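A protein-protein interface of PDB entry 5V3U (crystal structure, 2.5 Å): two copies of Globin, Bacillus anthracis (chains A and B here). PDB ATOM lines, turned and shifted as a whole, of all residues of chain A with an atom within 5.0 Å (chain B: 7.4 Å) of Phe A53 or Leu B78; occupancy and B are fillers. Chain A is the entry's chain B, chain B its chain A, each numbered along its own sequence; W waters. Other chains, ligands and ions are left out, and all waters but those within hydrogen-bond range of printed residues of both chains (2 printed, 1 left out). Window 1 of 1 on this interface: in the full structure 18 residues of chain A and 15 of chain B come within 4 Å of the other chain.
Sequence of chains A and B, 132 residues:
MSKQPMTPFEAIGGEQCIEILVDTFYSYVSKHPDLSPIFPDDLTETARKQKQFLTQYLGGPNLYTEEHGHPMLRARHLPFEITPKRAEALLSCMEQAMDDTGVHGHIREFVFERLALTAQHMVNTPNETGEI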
ATOM      1  N   LYS A  49      21.907   3.314 -34.620  1.00  0.00           N
ATOM      2  CA  LYS A  49      20.979   3.412 -33.501  1.00  0.00           C
ATOM      3  C   LYS A  49      19.526   3.407 -33.969  1.00  0.00           C
ATOM      4  O   LYS A  49      18.651   2.904 -33.255  1.00  0.00           O
ATOM      5  CB  LYS A  49      21.291   4.668 -32.678  1.00  0.00           C
ATOM      6  CG  LYS A  49      22.597   4.540 -31.915  1.00  0.00           C
ATOM      7  CD  LYS A  49      22.877   5.712 -31.004  1.00  0.00           C
ATOM      8  CE  LYS A  49      22.977   6.998 -31.786  1.00  0.00           C
ATOM      9  NZ  LYS A  49      23.736   7.992 -31.003  1.00  0.00           N
ATOM     10  N   GLN A  50      19.251   3.941 -35.160  1.00  0.00           N
ATOM     11  CA  GLN A  50      17.883   3.936 -35.668  1.00  0.00           C
ATOM     12  C   GLN A  50      17.437   2.524 -36.016  1.00  0.00           C
ATOM     13  O   GLN A  50      16.269   2.165 -35.818  1.00  0.00           O
ATOM     14  CB  GLN A  50      17.775   4.845 -36.885  1.00  0.00           C
ATOM     15  CG  GLN A  50      16.379   4.937 -37.439  1.00  0.00           C
ATOM     16  CD  GLN A  50      15.473   5.760 -36.532  1.00  0.00           C
ATOM     17  OE1 GLN A  50      14.821   5.261 -35.613  1.00  0.00           O
ATOM     18  NE2 GLN A  50      15.444   7.033 -36.790  1.00  0.00           N
ATOM     19  N   LYS A  51      18.359   1.718 -36.563  1.00  0.00           N
ATOM     20  CA  LYS A  51      18.109   0.295 -36.762  1.00  0.00           C
ATOM     21  C   LYS A  51      17.757  -0.375 -35.450  1.00  0.00           C
ATOM     22  O   LYS A  51      16.808  -1.170 -35.378  1.00  0.00           O
ATOM     23  CB  LYS A  51      19.334  -0.369 -37.380  1.00  0.00           C
ATOM     24  CG  LYS A  51      19.602   0.113 -38.773  1.00  0.00           C
ATOM     25  CD  LYS A  51      20.955  -0.304 -39.290  1.00  0.00           C
ATOM     26  CE  LYS A  51      21.252   0.441 -40.584  1.00  0.00           C
ATOM     27  NZ  LYS A  51      22.494  -0.081 -41.237  1.00  0.00           N
ATOM     28  N   GLN A  52      18.527  -0.073 -34.404  1.00  0.00           N
ATOM     29  CA  GLN A  52      18.200  -0.569 -33.076  1.00  0.00           C
ATOM     30  C   GLN A  52      16.808  -0.123 -32.660  1.00  0.00           C
ATOM     31  O   GLN A  52      15.977  -0.943 -32.252  1.00  0.00           O
ATOM     32  CB  GLN A  52      19.233  -0.084 -32.067  1.00  0.00           C
ATOM     33  CG  GLN A  52      20.633  -0.657 -32.240  1.00  0.00           C
ATOM     34  CD  GLN A  52      21.554  -0.163 -31.143  1.00  0.00           C
ATOM     35  OE1 GLN A  52      21.646   1.049 -30.895  1.00  0.00           O
ATOM     36  NE2 GLN A  52      22.202  -1.093 -30.445  1.00  0.00           N
ATOM     37  N   PHE A  53      16.527   1.175 -32.779  1.00  0.00           N
ATOM     38  CA  PHE A  53      15.252   1.679 -32.279  1.00  0.00           C
ATOM     39  C   PHE A  53      14.070   1.123 -33.071  1.00  0.00           C
ATOM     40  O   PHE A  53      13.055   0.748 -32.478  1.00  0.00           O
ATOM     41  CB  PHE A  53      15.222   3.209 -32.280  1.00  0.00           C
ATOM     42  CG  PHE A  53      14.104   3.766 -31.465  1.00  0.00           C
ATOM     43  CD1 PHE A  53      14.230   3.898 -30.091  1.00  0.00           C
ATOM     44  CD2 PHE A  53      12.895   4.106 -32.059  1.00  0.00           C
ATOM     45  CE1 PHE A  53      13.169   4.391 -29.328  1.00  0.00           C
ATOM     46  CE2 PHE A  53      11.838   4.594 -31.302  1.00  0.00           C
ATOM     47  CZ  PHE A  53      11.976   4.730 -29.937  1.00  0.00           C
ATOM     48  N   LEU A  54      14.163   1.064 -34.404  1.00  0.00           N
ATOM     49  CA  LEU A  54      13.012   0.583 -35.167  1.00  0.00           C
ATOM     50  C   LEU A  54      12.767  -0.899 -34.906  1.00  0.00           C
ATOM     51  O   LEU A  54      11.618  -1.337 -34.778  1.00  0.00           O
ATOM     52  CB  LEU A  54      13.204   0.862 -36.659  1.00  0.00           C
ATOM     53  CG  LEU A  54      13.278   2.363 -37.010  1.00  0.00           C
ATOM     54  CD1 LEU A  54      13.323   2.603 -38.515  1.00  0.00           C
ATOM     55  CD2 LEU A  54      12.104   3.131 -36.382  1.00  0.00           C
ATOM     56  N   THR A  55      13.840  -1.674 -34.778  1.00  0.00           N
ATOM     57  CA  THR A  55      13.691  -3.095 -34.490  1.00  0.00           C
ATOM     58  C   THR A  55      12.911  -3.317 -33.199  1.00  0.00           C
ATOM     59  O   THR A  55      12.035  -4.186 -33.138  1.00  0.00           O
ATOM     60  CB  THR A  55      15.073  -3.757 -34.427  1.00  0.00           C
ATOM     61  OG1 THR A  55      15.708  -3.691 -35.716  1.00  0.00           O
ATOM     62  CG2 THR A  55      14.961  -5.202 -33.989  1.00  0.00           C
ATOM     63  N   GLN A  56      13.203  -2.537 -32.157  1.00  0.00           N
ATOM     64  CA  GLN A  56      12.496  -2.729 -30.896  1.00  0.00           C
ATOM     65  C   GLN A  56      11.107  -2.115 -30.946  1.00  0.00           C
ATOM     66  O   GLN A  56      10.139  -2.726 -30.490  1.00  0.00           O
ATOM     67  CB  GLN A  56      13.304  -2.137 -29.744  1.00  0.00           C
ATOM     68  CG  GLN A  56      12.626  -2.236 -28.384  1.00  0.00           C
ATOM     69  CD  GLN A  56      13.559  -1.882 -27.242  1.00  0.00           C
ATOM     70  OE1 GLN A  56      14.706  -1.515 -27.463  1.00  0.00           O
ATOM     71  NE2 GLN A  56      13.075  -2.011 -26.018  1.00  0.00           N
ATOM     72  N   TYR A  57      10.985  -0.918 -31.514  1.00  0.00           N
ATOM     73  CA  TYR A  57       9.674  -0.295 -31.617  1.00  0.00           C
ATOM     74  C   TYR A  57       8.681  -1.206 -32.339  1.00  0.00           C
ATOM     75  O   TYR A  57       7.524  -1.331 -31.921  1.00  0.00           O
ATOM     76  CB  TYR A  57       9.800   1.057 -32.321  1.00  0.00           C
ATOM     77  CG  TYR A  57       8.487   1.790 -32.457  1.00  0.00           C
ATOM     78  CD1 TYR A  57       7.497   1.673 -31.480  1.00  0.00           C
ATOM     79  CD2 TYR A  57       8.224   2.580 -33.566  1.00  0.00           C
ATOM     80  CE1 TYR A  57       6.305   2.312 -31.602  1.00  0.00           C
ATOM     81  CE2 TYR A  57       7.019   3.234 -33.692  1.00  0.00           C
ATOM     82  CZ  TYR A  57       6.063   3.091 -32.706  1.00  0.00           C
ATOM     83  OH  TYR A  57       4.854   3.734 -32.825  1.00  0.00           O
ATOM     84  N   LEU A  58       9.117  -1.865 -33.410  1.00  0.00           N
ATOM     85  CA  LEU A  58       8.241  -2.700 -34.220  1.00  0.00           C
ATOM     86  C   LEU A  58       8.051  -4.092 -33.646  1.00  0.00           C
ATOM     87  O   LEU A  58       7.417  -4.930 -34.300  1.00  0.00           O
ATOM     88  CB  LEU A  58       8.791  -2.809 -35.648  1.00  0.00           C
ATOM     89  CG  LEU A  58       8.903  -1.517 -36.468  1.00  0.00           C
ATOM     90  CD1 LEU A  58       9.619  -1.775 -37.797  1.00  0.00           C
ATOM     91  CD2 LEU A  58       7.522  -0.898 -36.694  1.00  0.00           C
ATOM     92  N   TYR A  64      17.592  -1.417 -28.849  1.00  0.00           N
ATOM     93  CA  TYR A  64      17.916  -0.054 -28.442  1.00  0.00           C
ATOM     94  C   TYR A  64      18.060   0.054 -26.926  1.00  0.00           C
ATOM     95  O   TYR A  64      19.077   0.543 -26.423  1.00  0.00           O
ATOM     96  CB  TYR A  64      16.876   0.948 -28.952  1.00  0.00           C
ATOM     97  CG  TYR A  64      17.300   2.373 -28.638  1.00  0.00           C
ATOM     98  CD1 TYR A  64      17.019   2.949 -27.402  1.00  0.00           C
ATOM     99  CD2 TYR A  64      18.018   3.127 -29.551  1.00  0.00           C
ATOM    100  CE1 TYR A  64      17.432   4.229 -27.095  1.00  0.00           C
ATOM    101  CE2 TYR A  64      18.431   4.425 -29.248  1.00  0.00           C
ATOM    102  CZ  TYR A  64      18.132   4.960 -28.019  1.00  0.00           C
ATOM    103  OH  TYR A  64      18.531   6.226 -27.696  1.00  0.00           O
ATOM    104  N   THR A  65      17.044  -0.367 -26.172  1.00  0.00           N
ATOM    105  CA  THR A  65      17.117  -0.129 -24.737  1.00  0.00           C
ATOM    106  C   THR A  65      18.184  -0.982 -24.067  1.00  0.00           C
ATOM    107  O   THR A  65      18.676  -0.598 -23.003  1.00  0.00           O
ATOM    108  CB  THR A  65      15.751  -0.350 -24.078  1.00  0.00           C
ATOM    109  OG1 THR A  65      15.296  -1.690 -24.322  1.00  0.00           O
ATOM    110  CG2 THR A  65      14.742   0.627 -24.636  1.00  0.00           C
ATOM    111  N   PRO A  71      14.522   5.213 -23.592  1.00  0.00           N
ATOM    112  CA  PRO A  71      14.604   5.917 -24.884  1.00  0.00           C
ATOM    113  C   PRO A  71      14.484   7.428 -24.768  1.00  0.00           C
ATOM    114  O   PRO A  71      15.233   8.129 -25.449  1.00  0.00           O
ATOM    115  CB  PRO A  71      13.440   5.309 -25.679  1.00  0.00           C
ATOM    116  CG  PRO A  71      12.438   4.943 -24.623  1.00  0.00           C
ATOM    117  CD  PRO A  71      13.273   4.435 -23.466  1.00  0.00           C
ATOM    118  N   LEU A  73      12.825   9.774 -26.013  1.00  0.00           N
ATOM    119  CA  LEU A  73      13.168  10.162 -27.374  1.00  0.00           C
ATOM    120  C   LEU A  73      13.109  11.676 -27.568  1.00  0.00           C
ATOM    121  O   LEU A  73      14.045  12.278 -28.114  1.00  0.00           O
ATOM    122  CB  LEU A  73      12.229   9.458 -28.337  1.00  0.00           C
ATOM    123  CG  LEU A  73      12.678   9.394 -29.777  1.00  0.00           C
ATOM    124  CD1 LEU A  73      14.014   8.676 -29.863  1.00  0.00           C
ATOM    125  CD2 LEU A  73      11.616   8.690 -30.562  1.00  0.00           C
ATOM    126  N   MET B  72       2.546  -5.973 -26.792  1.00  0.00           N
ATOM    127  CA  MET B  72       3.912  -5.494 -26.556  1.00  0.00           C
ATOM    128  C   MET B  72       3.921  -4.015 -26.189  1.00  0.00           C
ATOM    129  O   MET B  72       4.574  -3.187 -26.826  1.00  0.00           O
ATOM    130  CB  MET B  72       4.792  -5.751 -27.774  1.00  0.00           C
ATOM    131  CG  MET B  72       5.418  -7.139 -27.822  1.00  0.00           C
ATOM    132  SD  MET B  72       6.247  -7.338 -29.403  1.00  0.00           S
ATOM    133  CE  MET B  72       7.323  -8.737 -29.100  1.00  0.00           C
ATOM    134  N   LEU B  73       3.156  -3.695 -25.145  1.00  0.00           N
ATOM    135  CA  LEU B  73       2.841  -2.298 -24.866  1.00  0.00           C
ATOM    136  C   LEU B  73       4.096  -1.480 -24.583  1.00  0.00           C
ATOM    137  O   LEU B  73       4.185  -0.314 -24.991  1.00  0.00           O
ATOM    138  CB  LEU B  73       1.852  -2.196 -23.704  1.00  0.00           C
ATOM    139  CG  LEU B  73       0.407  -2.595 -24.033  1.00  0.00           C
ATOM    140  CD1 LEU B  73      -0.518  -2.136 -22.946  1.00  0.00           C
ATOM    141  CD2 LEU B  73      -0.047  -2.027 -25.357  1.00  0.00           C
ATOM    142  N   ARG B  74       5.078  -2.067 -23.889  1.00  0.00           N
ATOM    143  CA  ARG B  74       6.297  -1.322 -23.605  1.00  0.00           C
ATOM    144  C   ARG B  74       6.970  -0.898 -24.890  1.00  0.00           C
ATOM    145  O   ARG B  74       7.423   0.247 -25.008  1.00  0.00           O
ATOM    146  CB  ARG B  74       7.254  -2.135 -22.738  1.00  0.00           C
ATOM    147  CG  ARG B  74       8.446  -1.325 -22.247  1.00  0.00           C
ATOM    148  CD  ARG B  74       9.459  -2.181 -21.489  1.00  0.00           C
ATOM    149  NE  ARG B  74      10.777  -1.543 -21.400  1.00  0.00           N
ATOM    150  CZ  ARG B  74      11.899  -2.027 -21.934  1.00  0.00           C
ATOM    151  NH1 ARG B  74      13.038  -1.366 -21.790  1.00  0.00           N
ATOM    152  NH2 ARG B  74      11.895  -3.177 -22.599  1.00  0.00           N
ATOM    153  N   ALA B  75       7.015  -1.791 -25.879  1.00  0.00           N
ATOM    154  CA  ALA B  75       7.615  -1.423 -27.157  1.00  0.00           C
ATOM    155  C   ALA B  75       6.802  -0.334 -27.850  1.00  0.00           C
ATOM    156  O   ALA B  75       7.370   0.640 -28.368  1.00  0.00           O
ATOM    157  CB  ALA B  75       7.760  -2.651 -28.060  1.00  0.00           C
ATOM    158  N   ARG B  76       5.472  -0.471 -27.853  1.00  0.00           N
ATOM    159  CA  ARG B  76       4.630   0.475 -28.573  1.00  0.00           C
ATOM    160  C   ARG B  76       4.641   1.876 -27.967  1.00  0.00           C
ATOM    161  O   ARG B  76       4.323   2.841 -28.671  1.00  0.00           O
ATOM    162  CB  ARG B  76       3.204  -0.049 -28.633  1.00  0.00           C
ATOM    163  CG  ARG B  76       3.044  -1.311 -29.453  1.00  0.00           C
ATOM    164  CD  ARG B  76       1.568  -1.617 -29.634  1.00  0.00           C
ATOM    165  NE  ARG B  76       1.330  -2.982 -30.091  1.00  0.00           N
ATOM    166  CZ  ARG B  76       1.113  -3.316 -31.357  1.00  0.00           C
ATOM    167  NH1 ARG B  76       0.899  -4.587 -31.686  1.00  0.00           N
ATOM    168  NH2 ARG B  76       1.116  -2.379 -32.295  1.00  0.00           N
ATOM    169  N   HIS B  77       4.993   2.014 -26.689  1.00  0.00           N
ATOM    170  CA  HIS B  77       5.013   3.307 -26.028  1.00  0.00           C
ATOM    171  C   HIS B  77       6.410   3.936 -26.006  1.00  0.00           C
ATOM    172  O   HIS B  77       6.582   5.037 -25.466  1.00  0.00           O
ATOM    173  CB  HIS B  77       4.456   3.181 -24.607  1.00  0.00           C
ATOM    174  CG  HIS B  77       2.956   3.101 -24.540  1.00  0.00           C
ATOM    175  ND1 HIS B  77       2.263   1.908 -24.606  1.00  0.00           N
ATOM    176  CD2 HIS B  77       2.019   4.064 -24.369  1.00  0.00           C
ATOM    177  CE1 HIS B  77       0.967   2.140 -24.493  1.00  0.00           C
ATOM    178  NE2 HIS B  77       0.790   3.440 -24.352  1.00  0.00           N
ATOM    179  N   LEU B  78       7.391   3.276 -26.624  1.00  0.00           N
ATOM    180  CA  LEU B  78       8.758   3.778 -26.676  1.00  0.00           C
ATOM    181  C   LEU B  78       8.907   5.201 -27.204  1.00  0.00           C
ATOM    182  O   LEU B  78       9.722   5.950 -26.635  1.00  0.00           O
ATOM    183  CB  LEU B  78       9.605   2.833 -27.534  1.00  0.00           C
ATOM    184  CG  LEU B  78      10.178   1.588 -26.873  1.00  0.00           C
ATOM    185  CD1 LEU B  78      11.127   0.897 -27.831  1.00  0.00           C
ATOM    186  CD2 LEU B  78      10.904   1.974 -25.607  1.00  0.00           C
ATOM    187  N   PRO B  79       8.222   5.632 -28.270  1.00  0.00           N
ATOM    188  CA  PRO B  79       8.510   6.968 -28.811  1.00  0.00           C
ATOM    189  C   PRO B  79       7.844   8.110 -28.060  1.00  0.00           C
ATOM    190  O   PRO B  79       8.183   9.267 -28.326  1.00  0.00           O
ATOM    191  CB  PRO B  79       7.986   6.889 -30.258  1.00  0.00           C
ATOM    192  CG  PRO B  79       7.330   5.525 -30.404  1.00  0.00           C
ATOM    193  CD  PRO B  79       7.164   4.960 -29.047  1.00  0.00           C
ATOM    194  N   PHE B  80       6.928   7.837 -27.138  1.00  0.00           N
ATOM    195  CA  PHE B  80       6.167   8.874 -26.454  1.00  0.00           C
ATOM    196  C   PHE B  80       6.808   9.239 -25.123  1.00  0.00           C
ATOM    197  O   PHE B  80       7.383   8.389 -24.441  1.00  0.00           O
ATOM    198  CB  PHE B  80       4.737   8.410 -26.237  1.00  0.00           C
ATOM    199  CG  PHE B  80       4.101   7.874 -27.469  1.00  0.00           C
ATOM    200  CD1 PHE B  80       4.262   8.524 -28.681  1.00  0.00           C
ATOM    201  CD2 PHE B  80       3.350   6.705 -27.428  1.00  0.00           C
ATOM    202  CE1 PHE B  80       3.675   8.024 -29.832  1.00  0.00           C
ATOM    203  CE2 PHE B  80       2.763   6.196 -28.572  1.00  0.00           C
ATOM    204  CZ  PHE B  80       2.921   6.851 -29.771  1.00  0.00           C
ATOM    205  N   GLU B  81       6.715  10.513 -24.759  1.00  0.00           N
ATOM    206  CA  GLU B  81       7.346  10.998 -23.535  1.00  0.00           C
ATOM    207  C   GLU B  81       6.446  10.596 -22.373  1.00  0.00           C
ATOM    208  O   GLU B  81       5.492  11.294 -22.023  1.00  0.00           O
ATOM    209  CB  GLU B  81       7.572  12.506 -23.601  1.00  0.00           C
ATOM    210  CG  GLU B  81       8.456  13.043 -22.475  1.00  0.00           C
ATOM    211  CD  GLU B  81       8.902  14.493 -22.681  1.00  0.00           C
ATOM    212  OE1 GLU B  81       8.034  15.405 -22.630  1.00  0.00           O
ATOM    213  OE2 GLU B  81      10.127  14.708 -22.891  1.00  0.00           O
ATOM    214  N   ILE B  82       6.745   9.443 -21.777  1.00  0.00           N
ATOM    215  CA  ILE B  82       5.966   8.905 -20.664  1.00  0.00           C
ATOM    216  C   ILE B  82       6.816   9.013 -19.403  1.00  0.00           C
ATOM    217  O   ILE B  82       7.680   8.168 -19.134  1.00  0.00           O
ATOM    218  CB  ILE B  82       5.515   7.463 -20.909  1.00  0.00           C
ATOM    219  CG1 ILE B  82       4.659   7.382 -22.185  1.00  0.00           C
ATOM    220  CG2 ILE B  82       4.748   6.966 -19.686  1.00  0.00           C
ATOM    221  CD1 ILE B  82       3.939   6.072 -22.381  1.00  0.00           C
ATOM    222  N   MET B 122       5.361   1.322 -18.696  1.00  0.00           N
ATOM    223  CA  MET B 122       5.391   2.232 -19.838  1.00  0.00           C
ATOM    224  C   MET B 122       6.363   3.397 -19.652  1.00  0.00           C
ATOM    225  O   MET B 122       6.821   3.958 -20.653  1.00  0.00           O
ATOM    226  CB  MET B 122       3.989   2.784 -20.141  1.00  0.00           C
ATOM    227  CG  MET B 122       2.876   1.747 -20.379  1.00  0.00           C
ATOM    228  SD  MET B 122       3.083   0.650 -21.808  1.00  0.00           S
ATOM    229  CE  MET B 122       4.010  -0.718 -21.078  1.00  0.00           C
ATOM    230  N   VAL B 123       6.713   3.748 -18.410  1.00  0.00           N
ATOM    231  CA  VAL B 123       7.547   4.925 -18.165  1.00  0.00           C
ATOM    232  C   VAL B 123       8.909   4.765 -18.836  1.00  0.00           C
ATOM    233  O   VAL B 123       9.602   3.755 -18.666  1.00  0.00           O
ATOM    234  CB  VAL B 123       7.684   5.180 -16.656  1.00  0.00           C
ATOM    235  CG1 VAL B 123       8.625   6.334 -16.403  1.00  0.00           C
ATOM    236  CG2 VAL B 123       6.314   5.461 -16.033  1.00  0.00           C
ATOM    237  N   ASN B 124       9.297   5.777 -19.601  1.00  0.00           N
ATOM    238  CA  ASN B 124      10.495   5.716 -20.417  1.00  0.00           C
ATOM    239  C   ASN B 124      11.255   7.044 -20.406  1.00  0.00           C
ATOM    240  O   ASN B 124      12.156   7.227 -21.235  1.00  0.00           O
ATOM    241  CB  ASN B 124      10.138   5.314 -21.854  1.00  0.00           C
ATOM    242  CG  ASN B 124       9.058   6.188 -22.464  1.00  0.00           C
ATOM    243  OD1 ASN B 124       8.930   7.374 -22.138  1.00  0.00           O
ATOM    244  ND2 ASN B 124       8.279   5.607 -23.369  1.00  0.00           N
ATOM    245  N   THR B 125      10.914   7.961 -19.482  1.00  0.00           N
ATOM    246  CA  THR B 125      11.504   9.279 -19.346  1.00  0.00           C
ATOM    247  C   THR B 125      11.612   9.587 -17.854  1.00  0.00           C
ATOM    248  O   THR B 125      10.610   9.463 -17.127  1.00  0.00           O
ATOM    249  CB  THR B 125      10.642  10.342 -20.046  1.00  0.00           C
ATOM    250  OG1 THR B 125      10.279   9.882 -21.353  1.00  0.00           O
ATOM    251  CG2 THR B 125      11.374  11.691 -20.147  1.00  0.00           C
HETATM  252  O   HOH W   1      15.405  -3.350 -21.454  1.00  0.00           O
HETATM  253  O   HOH W   2       9.728  10.996 -25.856  1.00  0.00           O
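Water W1 bridges NH1 of Arg B74 and OG1 of Thr A65. Water W2 lies within hydrogen-bond range of the backbone NH (N) of Glu B81, the backbone NH (N) of Leu A73 and the backbone carbonyl oxygen (O) of Pro B79.
CZ of Phe A53 touches CB of Leu B78, at 3.9 Å. NE2 of Gln A56 touches NH2 of Arg B74, at 3.8 Å. Gln A56 touches Ala B75 (O to CB, 3.4 Å). Gln A56 touches Leu B78. CD1 of Tyr A57 touches O of Ala B75, at 3.3 Å. Tyr A57 touches Arg B76. Pro B79 touches Tyr A57. Leu B78 touches Pro A71. Pro A71 touches Asn B124 (CG to CB, 3.6 Å). CA of Pro B79 touches CD2 of Leu A73, 3.96 Å away.
The backbone carbonyl oxygen of His B77 sits at hydrogen-bond distance from the side-chain amide nitrogen of Asn B124 (2.8 Å). The backbone carbonyl oxygen (O) of Phe B80 sits close to the side-chain amide oxygen (OD1) of Asn B124 (3.0 Å). O of Ile B82 sits at hydrogen-bond distance from N of Asn B124, 2.9 Å away. The side-chain amide nitrogen (ND2) of Asn B124 lies within hydrogen-bond range of the backbone carbonyl oxygen (O) of Met B122 (3.5 Å). The side-chain amide oxygen of Asn B124 lies within hydrogen-bond range of the side-chain hydroxyl of Thr B125 (3.0 Å). The side-chain amide nitrogen (NE2) of Gln A56 lies within hydrogen-bond range of the side-chain hydroxyl (OG1) of Thr A65, at 2.8 Å.
Printed residues of chain B that touch a printed residue of chain A: Arg B74, Ala B75, Arg B76, Leu B78, Pro B79 and Asn B124. Hydrophobic or aromatic side chains of chain B that line the printed part of chain A: Ala B75, Leu B78 and Pro B79. Of the 14 printed residues of chain A, 6 touch a printed residue of chain B. Printed residues of chain A that touch a printed residue of chain B: Phe A53, Gln A56, Tyr A57, Thr A65, Pro A71 and Leu A73.
OG1 of Thr A65 is in hydrogen-bond range of NH1 of Arg B74 (3.4 Å).
Leu B78 touches just these residues of chain A: Phe A53 (3.9 Å), Gln A56 (3.5 Å) and Pro A71 (3.5 Å). Of the printed residues of chain B, Gln A56 touches Arg B74 (3.8 Å), Ala B75 (3.4 Å) and Leu B78 (3.5 Å). Of the printed residues of chain B, Pro A71 touches Leu B78 and Asn B124. Printed residues of chain A within 4 Å of Ala B75: Gln A56 (3.4 Å) and Tyr A57 (3.3 Å). Gln A52 touches none of the printed residues of chain B. Leu B73 touches none of the printed residues of chain A. The nearest printed residue of chain B that does not touch Gln A56 is Arg B76 (5.8 Å).
Position printed for both chains: 73. Of the 11 pairs that touch across the chains among the printed residues, none has its exchanged pair printed and touching as well.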
